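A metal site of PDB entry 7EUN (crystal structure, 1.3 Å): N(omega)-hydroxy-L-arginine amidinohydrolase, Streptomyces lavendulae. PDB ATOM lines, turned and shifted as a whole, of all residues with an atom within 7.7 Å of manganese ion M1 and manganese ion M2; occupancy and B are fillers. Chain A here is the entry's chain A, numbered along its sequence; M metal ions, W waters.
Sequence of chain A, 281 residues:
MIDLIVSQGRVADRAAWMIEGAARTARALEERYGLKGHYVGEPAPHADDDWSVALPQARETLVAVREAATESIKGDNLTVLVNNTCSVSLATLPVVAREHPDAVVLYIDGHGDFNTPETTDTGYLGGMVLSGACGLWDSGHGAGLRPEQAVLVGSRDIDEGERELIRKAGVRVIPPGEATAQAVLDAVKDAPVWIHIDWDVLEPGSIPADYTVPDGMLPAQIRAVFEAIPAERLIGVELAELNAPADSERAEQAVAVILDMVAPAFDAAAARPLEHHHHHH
The side-chain carboxylate of Asp 200 sits close to the backbone NH of Gly 110 (3.1 Å).
The backbone NH (N) of Asp 198 is in hydrogen-bond range of the backbone carbonyl oxygen (O) of Ile 108, 2.9 Å away.
The side-chain hydroxyl (OH) of Tyr 107 lies close to the side-chain carboxylate (OD2) of Asp 113 (2.8 Å).
N of Val 129 lies within hydrogen-bond range of O of Asp 113.
OE2 of Glu 241 is in hydrogen-bond range of N of Cys 86, 2.8 Å away.
SG of Cys 86 sits close to NE2 of His 196.
Of the 23 residues printed, 4 come within 4 Å of manganese ion M1.
The nearest printed residue that does not touch manganese ion M1 is Tyr 107 (4.02 Å).
Of the 23 residues printed, 4 come within 4 Å of manganese ion M2.
Manganese ion M1 is bound by OD2 of Asp 109 (2.1 Å), OD2 of Asp 113 (2.2 Å), water W1 (2.2 Å), OD2 of Asp 198 (2.3 Å), water W2 (2.3 Å) and SG of Cys 86 (2.5 Å).
Manganese ion M2 is bound by the side-chain carboxylate (OD1) of Asp 109 (2.1 Å), the side-chain carboxylate (OD2) of Asp 200 (2.1 Å), water W2 (2.2 Å), the side-chain carboxylate (OD2) of Asp 198 (2.2 Å), a ring nitrogen (ND1) of His 111 (2.2 Å) and the side-chain carboxylate (OD1) of Asp 200 (2.4 Å).
Water W1 lies within hydrogen-bond range of the side-chain carboxylate (OE2) of Glu 241 (2.9 Å) and the backbone carbonyl oxygen (O) of Gly 126 (3.2 Å).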
ATOM      1  N   THR A  85     -15.226  -6.981  -6.855  1.00  0.00           N
ATOM      2  CA  THR A  85     -14.054  -6.474  -7.569  1.00  0.00           C
ATOM      3  C   THR A  85     -12.908  -7.483  -7.497  1.00  0.00           C
ATOM      4  O   THR A  85     -12.853  -8.334  -6.595  1.00  0.00           O
ATOM      5  CB  THR A  85     -13.574  -5.119  -6.977  1.00  0.00           C
ATOM      6  OG1 THR A  85     -13.178  -5.324  -5.628  1.00  0.00           O
ATOM      7  CG2 THR A  85     -14.663  -4.037  -7.046  1.00  0.00           C
ATOM      8  N   CYS A  86     -11.966  -7.335  -8.418  1.00  0.00           N
ATOM      9  CA  CYS A  86     -10.753  -8.143  -8.361  1.00  0.00           C
ATOM     10  C   CYS A  86      -9.995  -7.935  -7.058  1.00  0.00           C
ATOM     11  O   CYS A  86      -9.292  -8.836  -6.590  1.00  0.00           O
ATOM     12  CB  CYS A  86      -9.818  -7.834  -9.530  1.00  0.00           C
ATOM     13  SG  CYS A  86     -10.426  -8.474 -11.114  1.00  0.00           S
ATOM     14  N   SER A  87     -10.117  -6.751  -6.432  1.00  0.00           N
ATOM     15  CA  SER A  87      -9.347  -6.446  -5.234  1.00  0.00           C
ATOM     16  C   SER A  87      -9.688  -7.325  -4.053  1.00  0.00           C
ATOM     17  O   SER A  87      -8.872  -7.438  -3.122  1.00  0.00           O
ATOM     18  CB  SER A  87      -9.542  -4.972  -4.844  1.00  0.00           C
ATOM     19  OG  SER A  87      -9.041  -4.111  -5.842  1.00  0.00           O
ATOM     20  N   TYR A 107      -5.088 -15.971 -14.016  1.00  0.00           N
ATOM     21  CA  TYR A 107      -5.653 -14.636 -13.736  1.00  0.00           C
ATOM     22  C   TYR A 107      -6.178 -14.148 -15.078  1.00  0.00           C
ATOM     23  O   TYR A 107      -5.418 -13.648 -15.910  1.00  0.00           O
ATOM     24  CB  TYR A 107      -4.587 -13.767 -13.097  1.00  0.00           C
ATOM     25  CG  TYR A 107      -5.156 -12.535 -12.386  1.00  0.00           C
ATOM     26  CD1 TYR A 107      -5.578 -11.418 -13.120  1.00  0.00           C
ATOM     27  CD2 TYR A 107      -5.274 -12.479 -10.997  1.00  0.00           C
ATOM     28  CE1 TYR A 107      -6.096 -10.282 -12.473  1.00  0.00           C
ATOM     29  CE2 TYR A 107      -5.818 -11.352 -10.364  1.00  0.00           C
ATOM     30  CZ  TYR A 107      -6.191 -10.265 -11.092  1.00  0.00           C
ATOM     31  OH  TYR A 107      -6.722  -9.163 -10.437  1.00  0.00           O
ATOM     32  N   ILE A 108      -7.471 -14.352 -15.307  1.00  0.00           N
ATOM     33  CA  ILE A 108      -8.095 -14.155 -16.607  1.00  0.00           C
ATOM     34  C   ILE A 108      -8.712 -12.742 -16.575  1.00  0.00           C
ATOM     35  O   ILE A 108      -9.659 -12.481 -15.815  1.00  0.00           O
ATOM     36  CB  ILE A 108      -9.148 -15.242 -16.891  1.00  0.00           C
ATOM     37  CG1 ILE A 108      -8.577 -16.650 -16.648  1.00  0.00           C
ATOM     38  CG2 ILE A 108      -9.709 -15.071 -18.289  1.00  0.00           C
ATOM     39  CD1 ILE A 108      -9.519 -17.784 -17.022  1.00  0.00           C
ATOM     40  N   ASP A 109      -8.175 -11.814 -17.374  1.00  0.00           N
ATOM     41  CA  ASP A 109      -8.484 -10.392 -17.213  1.00  0.00           C
ATOM     42  C   ASP A 109      -8.035  -9.685 -18.478  1.00  0.00           C
ATOM     43  O   ASP A 109      -7.011 -10.045 -19.072  1.00  0.00           O
ATOM     44  CB  ASP A 109      -7.706  -9.878 -15.983  1.00  0.00           C
ATOM     45  CG  ASP A 109      -8.219  -8.537 -15.424  1.00  0.00           C
ATOM     46  OD1 ASP A 109      -8.533  -7.620 -16.249  1.00  0.00           O
ATOM     47  OD2 ASP A 109      -8.269  -8.440 -14.155  1.00  0.00           O
ATOM     48  N   GLY A 110      -8.812  -8.705 -18.942  1.00  0.00           N
ATOM     49  CA  GLY A 110      -8.325  -7.872 -20.040  1.00  0.00           C
ATOM     50  C   GLY A 110      -7.134  -7.010 -19.698  1.00  0.00           C
ATOM     51  O   GLY A 110      -6.434  -6.533 -20.610  1.00  0.00           O
ATOM     52  N   HIS A 111      -6.878  -6.814 -18.411  1.00  0.00           N
ATOM     53  CA  HIS A 111      -5.784  -6.034 -17.870  1.00  0.00           C
ATOM     54  C   HIS A 111      -4.747  -6.959 -17.215  1.00  0.00           C
ATOM     55  O   HIS A 111      -5.010  -8.128 -16.960  1.00  0.00           O
ATOM     56  CB  HIS A 111      -6.305  -5.075 -16.787  1.00  0.00           C
ATOM     57  CG  HIS A 111      -7.355  -4.135 -17.246  1.00  0.00           C
ATOM     58  ND1 HIS A 111      -8.704  -4.423 -17.172  1.00  0.00           N
ATOM     59  CD2 HIS A 111      -7.246  -2.919 -17.803  1.00  0.00           C
ATOM     60  CE1 HIS A 111      -9.382  -3.377 -17.640  1.00  0.00           C
ATOM     61  NE2 HIS A 111      -8.516  -2.462 -18.036  1.00  0.00           N
ATOM     62  N   GLY A 112      -3.603  -6.378 -16.861  1.00  0.00           N
ATOM     63  CA  GLY A 112      -2.605  -7.084 -16.096  1.00  0.00           C
ATOM     64  C   GLY A 112      -2.765  -7.016 -14.588  1.00  0.00           C
ATOM     65  O   GLY A 112      -2.246  -7.883 -13.859  1.00  0.00           O
ATOM     66  N   ASP A 113      -3.479  -5.985 -14.094  1.00  0.00           N
ATOM     67  CA  ASP A 113      -3.657  -5.765 -12.666  1.00  0.00           C
ATOM     68  C   ASP A 113      -2.336  -5.911 -11.919  1.00  0.00           C
ATOM     69  O   ASP A 113      -2.274  -6.479 -10.823  1.00  0.00           O
ATOM     70  CB  ASP A 113      -4.748  -6.655 -12.061  1.00  0.00           C
ATOM     71  CG  ASP A 113      -6.156  -6.316 -12.551  1.00  0.00           C
ATOM     72  OD1 ASP A 113      -6.305  -5.418 -13.404  1.00  0.00           O
ATOM     73  OD2 ASP A 113      -7.124  -6.950 -12.050  1.00  0.00           O
ATOM     74  N   TYR A 124      -5.919   3.318  -8.581  1.00  0.00           N
ATOM     75  CA  TYR A 124      -6.975   2.328  -8.366  1.00  0.00           C
ATOM     76  C   TYR A 124      -6.421   1.015  -7.829  1.00  0.00           C
ATOM     77  O   TYR A 124      -5.612   0.355  -8.490  1.00  0.00           O
ATOM     78  CB  TYR A 124      -7.765   2.138  -9.662  1.00  0.00           C
ATOM     79  CG  TYR A 124      -8.899   1.180  -9.552  1.00  0.00           C
ATOM     80  CD1 TYR A 124      -9.763   1.181  -8.465  1.00  0.00           C
ATOM     81  CD2 TYR A 124      -9.086   0.227 -10.540  1.00  0.00           C
ATOM     82  CE1 TYR A 124     -10.791   0.263  -8.378  1.00  0.00           C
ATOM     83  CE2 TYR A 124     -10.066  -0.702 -10.443  1.00  0.00           C
ATOM     84  CZ  TYR A 124     -10.929  -0.687  -9.375  1.00  0.00           C
ATOM     85  OH  TYR A 124     -11.875  -1.680  -9.350  1.00  0.00           O
ATOM     86  N   GLY A 126      -7.792  -1.832  -7.769  1.00  0.00           N
ATOM     87  CA  GLY A 126      -8.126  -2.928  -8.652  1.00  0.00           C
ATOM     88  C   GLY A 126      -7.115  -3.150  -9.739  1.00  0.00           C
ATOM     89  O   GLY A 126      -7.051  -4.251 -10.290  1.00  0.00           O
ATOM     90  N   GLY A 127      -6.277  -2.171 -10.021  1.00  0.00           N
ATOM     91  CA  GLY A 127      -5.182  -2.335 -10.954  1.00  0.00           C
ATOM     92  C   GLY A 127      -3.887  -2.823 -10.328  1.00  0.00           C
ATOM     93  O   GLY A 127      -2.875  -2.881 -11.025  1.00  0.00           O
ATOM     94  N   MET A 128      -3.906  -3.191  -9.043  1.00  0.00           N
ATOM     95  CA  MET A 128      -2.736  -3.519  -8.242  1.00  0.00           C
ATOM     96  C   MET A 128      -2.847  -4.895  -7.577  1.00  0.00           C
ATOM     97  O   MET A 128      -2.068  -5.211  -6.666  1.00  0.00           O
ATOM     98  CB  MET A 128      -2.559  -2.436  -7.154  1.00  0.00           C
ATOM     99  CG  MET A 128      -2.427  -1.007  -7.694  1.00  0.00           C
ATOM    100  SD  MET A 128      -2.696   0.305  -6.459  1.00  0.00           S
ATOM    101  CE  MET A 128      -1.258   0.067  -5.438  1.00  0.00           C
ATOM    102  N   VAL A 129      -3.801  -5.706  -8.016  1.00  0.00           N
ATOM    103  CA  VAL A 129      -4.160  -6.915  -7.267  1.00  0.00           C
ATOM    104  C   VAL A 129      -3.105  -8.004  -7.429  1.00  0.00           C
ATOM    105  O   VAL A 129      -2.652  -8.584  -6.443  1.00  0.00           O
ATOM    106  CB  VAL A 129      -5.545  -7.411  -7.744  1.00  0.00           C
ATOM    107  CG1 VAL A 129      -5.898  -8.722  -7.042  1.00  0.00           C
ATOM    108  CG2 VAL A 129      -6.588  -6.360  -7.507  1.00  0.00           C
ATOM    109  N   HIS A 196      -9.157 -17.157 -11.492  1.00  0.00           N
ATOM    110  CA  HIS A 196      -9.684 -15.830 -11.174  1.00  0.00           C
ATOM    111  C   HIS A 196     -10.120 -15.173 -12.482  1.00  0.00           C
ATOM    112  O   HIS A 196      -9.300 -15.024 -13.385  1.00  0.00           O
ATOM    113  CB  HIS A 196      -8.563 -15.008 -10.547  1.00  0.00           C
ATOM    114  CG  HIS A 196      -8.884 -13.562 -10.354  1.00  0.00           C
ATOM    115  ND1 HIS A 196      -9.136 -13.026  -9.101  1.00  0.00           N
ATOM    116  CD2 HIS A 196      -9.015 -12.535 -11.230  1.00  0.00           C
ATOM    117  CE1 HIS A 196      -9.419 -11.740  -9.225  1.00  0.00           C
ATOM    118  NE2 HIS A 196      -9.373 -11.412 -10.508  1.00  0.00           N
ATOM    119  N   ILE A 197     -11.391 -14.756 -12.592  1.00  0.00           N
ATOM    120  CA  ILE A 197     -11.884 -14.103 -13.799  1.00  0.00           C
ATOM    121  C   ILE A 197     -12.438 -12.712 -13.500  1.00  0.00           C
ATOM    122  O   ILE A 197     -13.300 -12.536 -12.628  1.00  0.00           O
ATOM    123  CB  ILE A 197     -12.963 -14.935 -14.513  1.00  0.00           C
ATOM    124  CG1 ILE A 197     -12.518 -16.333 -14.845  1.00  0.00           C
ATOM    125  CG2 ILE A 197     -13.364 -14.259 -15.808  1.00  0.00           C
ATOM    126  CD1 ILE A 197     -13.606 -17.221 -15.324  1.00  0.00           C
ATOM    127  N   ASP A 198     -11.963 -11.731 -14.272  1.00  0.00           N
ATOM    128  CA  ASP A 198     -12.534 -10.383 -14.395  1.00  0.00           C
ATOM    129  C   ASP A 198     -13.260 -10.354 -15.736  1.00  0.00           C
ATOM    130  O   ASP A 198     -12.636 -10.538 -16.776  1.00  0.00           O
ATOM    131  CB  ASP A 198     -11.367  -9.411 -14.384  1.00  0.00           C
ATOM    132  CG  ASP A 198     -11.728  -7.937 -14.621  1.00  0.00           C
ATOM    133  OD1 ASP A 198     -12.835  -7.652 -15.105  1.00  0.00           O
ATOM    134  OD2 ASP A 198     -10.816  -7.069 -14.384  1.00  0.00           O
ATOM    135  N   TRP A 199     -14.581 -10.127 -15.701  1.00  0.00           N
ATOM    136  CA  TRP A 199     -15.356 -10.220 -16.927  1.00  0.00           C
ATOM    137  C   TRP A 199     -14.968  -9.192 -17.995  1.00  0.00           C
ATOM    138  O   TRP A 199     -15.416  -9.353 -19.150  1.00  0.00           O
ATOM    139  CB  TRP A 199     -16.875 -10.141 -16.645  1.00  0.00           C
ATOM    140  CG  TRP A 199     -17.330 -11.248 -15.777  1.00  0.00           C
ATOM    141  CD1 TRP A 199     -17.924 -11.134 -14.566  1.00  0.00           C
ATOM    142  CD2 TRP A 199     -17.236 -12.671 -16.048  1.00  0.00           C
ATOM    143  NE1 TRP A 199     -18.191 -12.379 -14.039  1.00  0.00           N
ATOM    144  CE2 TRP A 199     -17.777 -13.337 -14.923  1.00  0.00           C
ATOM    145  CE3 TRP A 199     -16.764 -13.431 -17.110  1.00  0.00           C
ATOM    146  CZ2 TRP A 199     -17.866 -14.717 -14.843  1.00  0.00           C
ATOM    147  CZ3 TRP A 199     -16.810 -14.816 -17.005  1.00  0.00           C
ATOM    148  CH2 TRP A 199     -17.368 -15.450 -15.888  1.00  0.00           C
ATOM    149  N   ASP A 200     -14.186  -8.152 -17.676  1.00  0.00           N
ATOM    150  CA  ASP A 200     -13.725  -7.267 -18.740  1.00  0.00           C
ATOM    151  C   ASP A 200     -12.772  -7.971 -19.713  1.00  0.00           C
ATOM    152  O   ASP A 200     -12.410  -7.376 -20.735  1.00  0.00           O
ATOM    153  CB  ASP A 200     -13.160  -5.937 -18.244  1.00  0.00           C
ATOM    154  CG  ASP A 200     -11.880  -6.034 -17.447  1.00  0.00           C
ATOM    155  OD1 ASP A 200     -11.059  -6.983 -17.668  1.00  0.00           O
ATOM    156  OD2 ASP A 200     -11.606  -5.133 -16.617  1.00  0.00           O
ATOM    157  N   VAL A 201     -12.410  -9.233 -19.461  1.00  0.00           N
ATOM    158  CA  VAL A 201     -11.653  -9.980 -20.452  1.00  0.00           C
ATOM    159  C   VAL A 201     -12.476 -10.230 -21.714  1.00  0.00           C
ATOM    160  O   VAL A 201     -11.901 -10.479 -22.793  1.00  0.00           O
ATOM    161  CB  VAL A 201     -11.127 -11.299 -19.850  1.00  0.00           C
ATOM    162  CG1 VAL A 201     -12.251 -12.322 -19.681  1.00  0.00           C
ATOM    163  CG2 VAL A 201      -9.977 -11.890 -20.668  1.00  0.00           C
ATOM    164  N   ALA A 240     -15.468 -12.203 -10.870  1.00  0.00           N
ATOM    165  CA  ALA A 240     -15.419 -10.804 -10.432  1.00  0.00           C
ATOM    166  C   ALA A 240     -15.795  -9.822 -11.537  1.00  0.00           C
ATOM    167  O   ALA A 240     -15.566 -10.066 -12.726  1.00  0.00           O
ATOM    168  CB  ALA A 240     -14.012 -10.434  -9.937  1.00  0.00           C
ATOM    169  N   GLU A 241     -16.375  -8.689 -11.108  1.00  0.00           N
ATOM    170  CA  GLU A 241     -16.500  -7.477 -11.934  1.00  0.00           C
ATOM    171  C   GLU A 241     -17.587  -7.617 -13.007  1.00  0.00           C
ATOM    172  O   GLU A 241     -17.400  -7.233 -14.159  1.00  0.00           O
ATOM    173  CB  GLU A 241     -15.149  -7.038 -12.516  1.00  0.00           C
ATOM    174  CG  GLU A 241     -14.099  -6.893 -11.426  1.00  0.00           C
ATOM    175  CD  GLU A 241     -13.266  -5.621 -11.429  1.00  0.00           C
ATOM    176  OE1 GLU A 241     -13.390  -4.817 -12.358  1.00  0.00           O
ATOM    177  OE2 GLU A 241     -12.451  -5.473 -10.473  1.00  0.00           O
HETATM  178 MN    MN M   1      -9.204  -7.074 -12.808  1.00  0.00          MN
HETATM  179 MN    MN M   2      -9.748  -5.989 -15.965  1.00  0.00          MN
HETATM  180  O   HOH W   1      -9.777  -5.303 -11.598  1.00  0.00           O
HETATM  181  O   HOH W   2      -8.767  -5.258 -14.195  1.00  0.00           O
